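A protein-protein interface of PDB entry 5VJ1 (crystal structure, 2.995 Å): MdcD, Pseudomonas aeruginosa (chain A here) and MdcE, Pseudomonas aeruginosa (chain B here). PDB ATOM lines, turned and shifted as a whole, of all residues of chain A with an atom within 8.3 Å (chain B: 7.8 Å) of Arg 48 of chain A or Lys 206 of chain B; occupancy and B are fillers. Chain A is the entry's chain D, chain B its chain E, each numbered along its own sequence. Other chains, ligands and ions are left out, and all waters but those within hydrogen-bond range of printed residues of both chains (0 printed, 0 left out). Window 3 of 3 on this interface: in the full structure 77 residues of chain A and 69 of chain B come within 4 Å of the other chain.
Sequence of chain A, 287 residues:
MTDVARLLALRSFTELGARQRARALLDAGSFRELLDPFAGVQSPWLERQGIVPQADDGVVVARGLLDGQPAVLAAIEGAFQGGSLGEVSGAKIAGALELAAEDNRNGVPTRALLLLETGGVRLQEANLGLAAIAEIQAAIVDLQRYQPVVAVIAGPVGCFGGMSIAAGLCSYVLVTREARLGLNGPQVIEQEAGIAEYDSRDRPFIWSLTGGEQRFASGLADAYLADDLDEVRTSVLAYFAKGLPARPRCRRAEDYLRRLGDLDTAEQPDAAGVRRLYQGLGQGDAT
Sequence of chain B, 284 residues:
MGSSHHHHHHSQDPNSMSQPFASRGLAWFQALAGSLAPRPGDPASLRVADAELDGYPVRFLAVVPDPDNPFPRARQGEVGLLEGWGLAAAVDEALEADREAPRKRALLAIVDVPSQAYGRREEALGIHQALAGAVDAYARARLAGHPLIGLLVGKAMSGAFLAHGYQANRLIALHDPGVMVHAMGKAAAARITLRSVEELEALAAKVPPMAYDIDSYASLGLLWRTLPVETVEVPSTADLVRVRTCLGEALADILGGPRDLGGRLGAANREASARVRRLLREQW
The guanidinium group (NH1) of Arg 48 of chain A is in hydrogen-bond range of the backbone carbonyl oxygen (O) of Lys 206 of chain B (3.3 Å).
The guanidinium group of Arg 195 of chain B lies within hydrogen-bond range of the side-chain amide oxygen of Gln 49 of chain A, 3.1 Å away.
OE1 of Gln 49 of chain A sits close to SD of Met 210 of chain B (3.6 Å).
The backbone carbonyl oxygen (O) of Gln 124 of chain A lies close to the side-chain sulfur (SD) of Met 210 of chain B, at 3.6 Å.
The backbone NH of Trp 45 of chain A sits close to the side-chain hydroxyl of Ser 43 of chain A.
The backbone carbonyl oxygen of Pro 44 of chain A lies within hydrogen-bond range of the guanidinium group of Arg 48 of chain A, 3.5 Å away.
The backbone carbonyl oxygen of Trp 45 of chain A is in hydrogen-bond range of the side-chain amide nitrogen of Gln 49 of chain A, at 2.9 Å.
The backbone carbonyl oxygen (O) of Leu 46 of chain A is in hydrogen-bond range of the backbone NH (N) of Ile 51 of chain A (3.2 Å).
The side-chain amide nitrogen (NE2) of Gln 49 of chain A is in hydrogen-bond range of the backbone carbonyl oxygen (O) of Gln 124 of chain A (2.8 Å).
Among the printed residues, merely in contact across the chains: Trp 45 of chain A with Asn 269 of chain B (3.2 Å), Ile 51 of chain A with Arg 195 of chain B (3.4 Å), Gln 49 of chain A with Val 207 of chain B (3.5 Å), Gln 124 of chain A with Arg 195 of chain B (3.5 Å), Trp 45 of chain A with Pro 209 of chain B (3.6 Å), Arg 48 of chain A with Val 207 of chain B (3.7 Å) and Gln 49 of chain A with Leu 203 of chain B (3.97 Å).
Of chain B, only Lys 206 and Val 207 come within 4 Å of Arg 48 of chain A.
No residue of chain A comes within 4 Å of Ala 205 of chain B.
Of the printed residues of chain A, Asn 269 of chain B touches Trp 45.
Of the printed residues of chain B, Gln 49 of chain A touches Arg 195, Leu 203, Val 207 and Met 210.
Val 52 of chain A touches none of the printed residues of chain B.
The nearest residue of chain A that does not touch Lys 206 of chain B is Trp 45 of chain A (5.7 Å).
The nearest printed residue of chain B that does not touch Gln 124 of chain A is Val 207 of chain B (4.2 Å).
Printed residues of chain B that touch a printed residue of chain A: Arg 195, Leu 203, Lys 206, Val 207, Pro 209, Met 210 and Asn 269.
Along chain B the printed residues that touch a printed residue of chain A span positions 195 to 269.
Of the 12 printed residues of chain A, 5 touch a printed residue of chain B.
Hydrophobic or aromatic side chains of chain A that line the printed part of chain B: Trp 45 and Ile 51.
Among the printed residues, 11 pairs touch across the chains.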
ATOM      1  N   SER A  43     -10.934  22.137  32.012  1.00  0.00           N
ATOM      2  CA  SER A  43      -9.504  22.387  31.964  1.00  0.00           C
ATOM      3  C   SER A  43      -9.124  23.728  31.331  1.00  0.00           C
ATOM      4  O   SER A  43      -9.459  24.008  30.184  1.00  0.00           O
ATOM      5  CB  SER A  43      -8.822  21.260  31.206  1.00  0.00           C
ATOM      6  OG  SER A  43      -7.507  21.641  30.880  1.00  0.00           O
ATOM      7  N   PRO A  44      -8.391  24.557  32.077  1.00  0.00           N
ATOM      8  CA  PRO A  44      -7.984  25.848  31.523  1.00  0.00           C
ATOM      9  C   PRO A  44      -6.765  25.755  30.600  1.00  0.00           C
ATOM     10  O   PRO A  44      -6.299  26.775  30.076  1.00  0.00           O
ATOM     11  CB  PRO A  44      -7.648  26.655  32.777  1.00  0.00           C
ATOM     12  CG  PRO A  44      -7.149  25.615  33.727  1.00  0.00           C
ATOM     13  CD  PRO A  44      -8.070  24.456  33.514  1.00  0.00           C
ATOM     14  N   TRP A  45      -6.272  24.549  30.355  1.00  0.00           N
ATOM     15  CA  TRP A  45      -5.041  24.446  29.587  1.00  0.00           C
ATOM     16  C   TRP A  45      -5.195  23.772  28.237  1.00  0.00           C
ATOM     17  O   TRP A  45      -4.229  23.699  27.483  1.00  0.00           O
ATOM     18  CB  TRP A  45      -3.974  23.680  30.382  1.00  0.00           C
ATOM     19  CG  TRP A  45      -3.845  24.140  31.767  1.00  0.00           C
ATOM     20  CD1 TRP A  45      -4.404  23.577  32.868  1.00  0.00           C
ATOM     21  CD2 TRP A  45      -3.170  25.325  32.211  1.00  0.00           C
ATOM     22  NE1 TRP A  45      -4.082  24.310  33.981  1.00  0.00           N
ATOM     23  CE2 TRP A  45      -3.335  25.387  33.605  1.00  0.00           C
ATOM     24  CE3 TRP A  45      -2.434  26.320  31.566  1.00  0.00           C
ATOM     25  CZ2 TRP A  45      -2.778  26.413  34.367  1.00  0.00           C
ATOM     26  CZ3 TRP A  45      -1.886  27.334  32.324  1.00  0.00           C
ATOM     27  CH2 TRP A  45      -2.061  27.372  33.715  1.00  0.00           C
ATOM     28  N   LEU A  46      -6.389  23.291  27.914  1.00  0.00           N
ATOM     29  CA  LEU A  46      -6.521  22.496  26.704  1.00  0.00           C
ATOM     30  C   LEU A  46      -6.824  23.308  25.449  1.00  0.00           C
ATOM     31  O   LEU A  46      -6.135  23.127  24.451  1.00  0.00           O
ATOM     32  CB  LEU A  46      -7.587  21.425  26.887  1.00  0.00           C
ATOM     33  CG  LEU A  46      -7.268  20.268  27.833  1.00  0.00           C
ATOM     34  CD1 LEU A  46      -8.459  19.324  27.857  1.00  0.00           C
ATOM     35  CD2 LEU A  46      -6.000  19.550  27.410  1.00  0.00           C
ATOM     36  N   GLU A  47      -7.815  24.204  25.498  1.00  0.00           N
ATOM     37  CA  GLU A  47      -8.191  25.031  24.333  1.00  0.00           C
ATOM     38  C   GLU A  47      -6.990  25.759  23.694  1.00  0.00           C
ATOM     39  O   GLU A  47      -6.865  25.818  22.470  1.00  0.00           O
ATOM     40  CB  GLU A  47      -9.238  26.051  24.746  1.00  0.00           C
ATOM     41  CG  GLU A  47     -10.389  25.434  25.477  1.00  0.00           C
ATOM     42  CD  GLU A  47     -11.091  26.426  26.395  1.00  0.00           C
ATOM     43  OE1 GLU A  47     -10.378  27.057  27.226  1.00  0.00           O
ATOM     44  OE2 GLU A  47     -12.339  26.571  26.281  1.00  0.00           O
ATOM     45  N   ARG A  48      -6.115  26.310  24.528  1.00  0.00           N
ATOM     46  CA  ARG A  48      -4.947  27.032  24.042  1.00  0.00           C
ATOM     47  C   ARG A  48      -4.020  26.126  23.216  1.00  0.00           C
ATOM     48  O   ARG A  48      -3.272  26.605  22.377  1.00  0.00           O
ATOM     49  CB  ARG A  48      -4.181  27.646  25.216  1.00  0.00           C
ATOM     50  CG  ARG A  48      -3.476  26.619  26.107  1.00  0.00           C
ATOM     51  CD  ARG A  48      -2.751  27.296  27.237  1.00  0.00           C
ATOM     52  NE  ARG A  48      -3.683  27.985  28.123  1.00  0.00           N
ATOM     53  CZ  ARG A  48      -3.309  28.918  28.986  1.00  0.00           C
ATOM     54  NH1 ARG A  48      -2.027  29.260  29.046  1.00  0.00           N
ATOM     55  NH2 ARG A  48      -4.203  29.513  29.766  1.00  0.00           N
ATOM     56  N   GLN A  49      -4.057  24.822  23.473  1.00  0.00           N
ATOM     57  CA  GLN A  49      -3.242  23.861  22.733  1.00  0.00           C
ATOM     58  C   GLN A  49      -3.990  23.234  21.562  1.00  0.00           C
ATOM     59  O   GLN A  49      -3.476  22.301  20.933  1.00  0.00           O
ATOM     60  CB  GLN A  49      -2.781  22.720  23.633  1.00  0.00           C
ATOM     61  CG  GLN A  49      -2.300  23.106  25.001  1.00  0.00           C
ATOM     62  CD  GLN A  49      -1.842  21.896  25.779  1.00  0.00           C
ATOM     63  OE1 GLN A  49      -1.521  20.846  25.195  1.00  0.00           O
ATOM     64  NE2 GLN A  49      -1.859  22.008  27.107  1.00  0.00           N
ATOM     65  N   GLY A  50      -5.212  23.692  21.296  1.00  0.00           N
ATOM     66  CA  GLY A  50      -5.999  23.111  20.223  1.00  0.00           C
ATOM     67  C   GLY A  50      -6.564  21.736  20.531  1.00  0.00           C
ATOM     68  O   GLY A  50      -6.818  20.930  19.632  1.00  0.00           O
ATOM     69  N   ILE A  51      -6.773  21.489  21.815  1.00  0.00           N
ATOM     70  CA  ILE A  51      -7.417  20.283  22.313  1.00  0.00           C
ATOM     71  C   ILE A  51      -8.805  20.596  22.857  1.00  0.00           C
ATOM     72  O   ILE A  51      -8.967  21.495  23.671  1.00  0.00           O
ATOM     73  CB  ILE A  51      -6.589  19.628  23.409  1.00  0.00           C
ATOM     74  CG1 ILE A  51      -5.293  19.085  22.816  1.00  0.00           C
ATOM     75  CG2 ILE A  51      -7.352  18.500  24.047  1.00  0.00           C
ATOM     76  CD1 ILE A  51      -4.361  18.489  23.847  1.00  0.00           C
ATOM     77  N   VAL A  52      -9.815  19.878  22.385  1.00  0.00           N
ATOM     78  CA  VAL A  52     -11.172  20.121  22.851  1.00  0.00           C
ATOM     79  C   VAL A  52     -11.357  19.589  24.260  1.00  0.00           C
ATOM     80  O   VAL A  52     -11.029  18.442  24.523  1.00  0.00           O
ATOM     81  CB  VAL A  52     -12.191  19.497  21.909  1.00  0.00           C
ATOM     82  CG1 VAL A  52     -13.608  19.793  22.382  1.00  0.00           C
ATOM     83  CG2 VAL A  52     -11.948  20.027  20.509  1.00  0.00           C
ATOM     84  N   PRO A  53     -11.863  20.432  25.175  1.00  0.00           N
ATOM     85  CA  PRO A  53     -12.017  20.060  26.583  1.00  0.00           C
ATOM     86  C   PRO A  53     -13.337  19.380  26.875  1.00  0.00           C
ATOM     87  O   PRO A  53     -14.272  19.607  26.123  1.00  0.00           O
ATOM     88  CB  PRO A  53     -11.938  21.414  27.291  1.00  0.00           C
ATOM     89  CG  PRO A  53     -12.603  22.318  26.352  1.00  0.00           C
ATOM     90  CD  PRO A  53     -12.135  21.866  24.978  1.00  0.00           C
ATOM     91  N   GLN A 124      -0.324  16.727  28.863  1.00  0.00           N
ATOM     92  CA  GLN A 124      -0.618  18.041  28.286  1.00  0.00           C
ATOM     93  C   GLN A 124      -0.834  19.066  29.371  1.00  0.00           C
ATOM     94  O   GLN A 124      -1.061  20.234  29.081  1.00  0.00           O
ATOM     95  CB  GLN A 124      -1.863  18.021  27.404  1.00  0.00           C
ATOM     96  CG  GLN A 124      -1.751  17.239  26.117  1.00  0.00           C
ATOM     97  CD  GLN A 124      -2.267  15.840  26.266  1.00  0.00           C
ATOM     98  OE1 GLN A 124      -2.543  15.392  27.379  1.00  0.00           O
ATOM     99  NE2 GLN A 124      -2.428  15.140  25.145  1.00  0.00           N
ATOM    100  N   ARG B 195       2.685  13.774  19.286  1.00  0.00           N
ATOM    101  CA  ARG B 195       3.279  15.061  18.951  1.00  0.00           C
ATOM    102  C   ARG B 195       4.783  14.870  18.725  1.00  0.00           C
ATOM    103  O   ARG B 195       5.349  13.862  19.157  1.00  0.00           O
ATOM    104  CB  ARG B 195       3.036  16.079  20.066  1.00  0.00           C
ATOM    105  CG  ARG B 195       1.583  16.491  20.239  1.00  0.00           C
ATOM    106  CD  ARG B 195       1.395  17.363  21.465  1.00  0.00           C
ATOM    107  NE  ARG B 195       0.139  18.085  21.375  1.00  0.00           N
ATOM    108  CZ  ARG B 195      -0.429  18.733  22.383  1.00  0.00           C
ATOM    109  NH1 ARG B 195       0.142  18.755  23.582  1.00  0.00           N
ATOM    110  NH2 ARG B 195      -1.584  19.353  22.184  1.00  0.00           N
ATOM    111  N   LEU B 200       6.257  19.922  21.428  1.00  0.00           N
ATOM    112  CA  LEU B 200       6.270  19.980  22.900  1.00  0.00           C
ATOM    113  C   LEU B 200       7.011  21.240  23.361  1.00  0.00           C
ATOM    114  O   LEU B 200       6.413  22.132  23.964  1.00  0.00           O
ATOM    115  CB  LEU B 200       6.910  18.740  23.526  1.00  0.00           C
ATOM    116  CG  LEU B 200       6.228  17.399  23.270  1.00  0.00           C
ATOM    117  CD1 LEU B 200       6.840  16.321  24.154  1.00  0.00           C
ATOM    118  CD2 LEU B 200       4.732  17.505  23.463  1.00  0.00           C
ATOM    119  N   GLU B 201       8.314  21.295  23.097  1.00  0.00           N
ATOM    120  CA  GLU B 201       9.131  22.457  23.443  1.00  0.00           C
ATOM    121  C   GLU B 201       8.493  23.770  22.983  1.00  0.00           C
ATOM    122  O   GLU B 201       8.593  24.794  23.659  1.00  0.00           O
ATOM    123  CB  GLU B 201      10.537  22.293  22.864  1.00  0.00           C
ATOM    124  CG  GLU B 201      11.306  21.121  23.498  1.00  0.00           C
ATOM    125  CD  GLU B 201      12.705  20.925  22.918  1.00  0.00           C
ATOM    126  OE1 GLU B 201      13.410  21.947  22.741  1.00  0.00           O
ATOM    127  OE2 GLU B 201      13.105  19.755  22.667  1.00  0.00           O
ATOM    128  N   ALA B 202       7.800  23.719  21.853  1.00  0.00           N
ATOM    129  CA  ALA B 202       7.030  24.861  21.366  1.00  0.00           C
ATOM    130  C   ALA B 202       5.938  25.179  22.373  1.00  0.00           C
ATOM    131  O   ALA B 202       5.936  26.243  23.009  1.00  0.00           O
ATOM    132  CB  ALA B 202       6.430  24.568  19.994  1.00  0.00           C
ATOM    133  N   LEU B 203       4.996  24.245  22.480  1.00  0.00           N
ATOM    134  CA  LEU B 203       3.928  24.282  23.471  1.00  0.00           C
ATOM    135  C   LEU B 203       4.400  24.551  24.899  1.00  0.00           C
ATOM    136  O   LEU B 203       3.687  25.195  25.662  1.00  0.00           O
ATOM    137  CB  LEU B 203       3.157  22.965  23.432  1.00  0.00           C
ATOM    138  CG  LEU B 203       2.181  22.830  22.265  1.00  0.00           C
ATOM    139  CD1 LEU B 203       1.264  21.649  22.489  1.00  0.00           C
ATOM    140  CD2 LEU B 203       1.367  24.102  22.081  1.00  0.00           C
ATOM    141  N   ALA B 204       5.614  24.127  25.250  1.00  0.00           N
ATOM    142  CA  ALA B 204       6.046  24.183  26.649  1.00  0.00           C
ATOM    143  C   ALA B 204       6.292  25.616  27.089  1.00  0.00           C
ATOM    144  O   ALA B 204       6.451  25.893  28.273  1.00  0.00           O
ATOM    145  CB  ALA B 204       7.296  23.353  26.862  1.00  0.00           C
ATOM    146  N   ALA B 205       6.285  26.532  26.132  1.00  0.00           N
ATOM    147  CA  ALA B 205       6.463  27.943  26.416  1.00  0.00           C
ATOM    148  C   ALA B 205       5.121  28.647  26.579  1.00  0.00           C
ATOM    149  O   ALA B 205       5.020  29.713  27.175  1.00  0.00           O
ATOM    150  CB  ALA B 205       7.254  28.579  25.322  1.00  0.00           C
ATOM    151  N   LYS B 206       4.093  28.050  26.004  1.00  0.00           N
ATOM    152  CA  LYS B 206       2.760  28.631  25.975  1.00  0.00           C
ATOM    153  C   LYS B 206       1.875  28.065  27.095  1.00  0.00           C
ATOM    154  O   LYS B 206       0.827  28.633  27.451  1.00  0.00           O
ATOM    155  CB  LYS B 206       2.147  28.340  24.592  1.00  0.00           C
ATOM    156  CG  LYS B 206       0.943  29.175  24.166  1.00  0.00           C
ATOM    157  CD  LYS B 206       0.709  29.033  22.653  1.00  0.00           C
ATOM    158  CE  LYS B 206       1.983  29.418  21.867  1.00  0.00           C
ATOM    159  NZ  LYS B 206       2.561  30.762  22.239  1.00  0.00           N
ATOM    160  N   VAL B 207       2.305  26.919  27.622  1.00  0.00           N
ATOM    161  CA  VAL B 207       1.577  26.191  28.650  1.00  0.00           C
ATOM    162  C   VAL B 207       2.539  25.835  29.780  1.00  0.00           C
ATOM    163  O   VAL B 207       3.183  24.776  29.752  1.00  0.00           O
ATOM    164  CB  VAL B 207       0.924  24.890  28.075  1.00  0.00           C
ATOM    165  CG1 VAL B 207      -0.044  24.269  29.071  1.00  0.00           C
ATOM    166  CG2 VAL B 207       0.212  25.169  26.779  1.00  0.00           C
ATOM    167  N   PRO B 208       2.657  26.720  30.772  1.00  0.00           N
ATOM    168  CA  PRO B 208       3.585  26.536  31.889  1.00  0.00           C
ATOM    169  C   PRO B 208       3.507  25.139  32.526  1.00  0.00           C
ATOM    170  O   PRO B 208       4.536  24.578  32.910  1.00  0.00           O
ATOM    171  CB  PRO B 208       3.163  27.630  32.864  1.00  0.00           C
ATOM    172  CG  PRO B 208       2.638  28.689  31.974  1.00  0.00           C
ATOM    173  CD  PRO B 208       1.859  27.940  30.936  1.00  0.00           C
ATOM    174  N   PRO B 209       2.300  24.578  32.684  1.00  0.00           N
ATOM    175  CA  PRO B 209       2.420  23.256  33.303  1.00  0.00           C
ATOM    176  C   PRO B 209       3.088  22.191  32.430  1.00  0.00           C
ATOM    177  O   PRO B 209       3.311  21.098  32.931  1.00  0.00           O
ATOM    178  CB  PRO B 209       0.955  22.898  33.614  1.00  0.00           C
ATOM    179  CG  PRO B 209       0.141  23.755  32.705  1.00  0.00           C
ATOM    180  CD  PRO B 209       0.899  25.039  32.649  1.00  0.00           C
ATOM    181  N   MET B 210       3.408  22.493  31.175  1.00  0.00           N
ATOM    182  CA  MET B 210       4.027  21.515  30.282  1.00  0.00           C
ATOM    183  C   MET B 210       5.541  21.658  30.236  1.00  0.00           C
ATOM    184  O   MET B 210       6.245  20.792  29.715  1.00  0.00           O
ATOM    185  CB  MET B 210       3.475  21.669  28.872  1.00  0.00           C
ATOM    186  CG  MET B 210       2.242  20.840  28.579  1.00  0.00           C
ATOM    187  SD  MET B 210       1.728  20.871  26.846  1.00  0.00           S
ATOM    188  CE  MET B 210       2.795  19.617  26.150  1.00  0.00           C
ATOM    189  N   ALA B 211       6.036  22.770  30.768  1.00  0.00           N
ATOM    190  CA  ALA B 211       7.449  23.110  30.664  1.00  0.00           C
ATOM    191  C   ALA B 211       8.281  22.351  31.681  1.00  0.00           C
ATOM    192  O   ALA B 211       7.773  21.937  32.724  1.00  0.00           O
ATOM    193  CB  ALA B 211       7.635  24.616  30.829  1.00  0.00           C
ATOM    194  N   SER B 216       9.084  27.928  35.198  1.00  0.00           N
ATOM    195  CA  SER B 216       7.720  27.542  34.910  1.00  0.00           C
ATOM    196  C   SER B 216       7.114  26.758  36.069  1.00  0.00           C
ATOM    197  O   SER B 216       5.912  26.840  36.321  1.00  0.00           O
ATOM    198  CB  SER B 216       7.669  26.728  33.631  1.00  0.00           C
ATOM    199  OG  SER B 216       7.863  27.563  32.508  1.00  0.00           O
ATOM    200  N   ASN B 269      -1.754  30.491  38.626  1.00  0.00           N
ATOM    201  CA  ASN B 269      -1.807  29.392  37.673  1.00  0.00           C
ATOM    202  C   ASN B 269      -2.494  28.146  38.225  1.00  0.00           C
ATOM    203  O   ASN B 269      -2.882  27.253  37.455  1.00  0.00           O
ATOM    204  CB  ASN B 269      -0.417  29.023  37.159  1.00  0.00           C
ATOM    205  CG  ASN B 269       0.111  30.025  36.167  1.00  0.00           C
ATOM    206  OD1 ASN B 269      -0.667  30.711  35.500  1.00  0.00           O
ATOM    207  ND2 ASN B 269       1.417  30.027  35.965  1.00  0.00           N
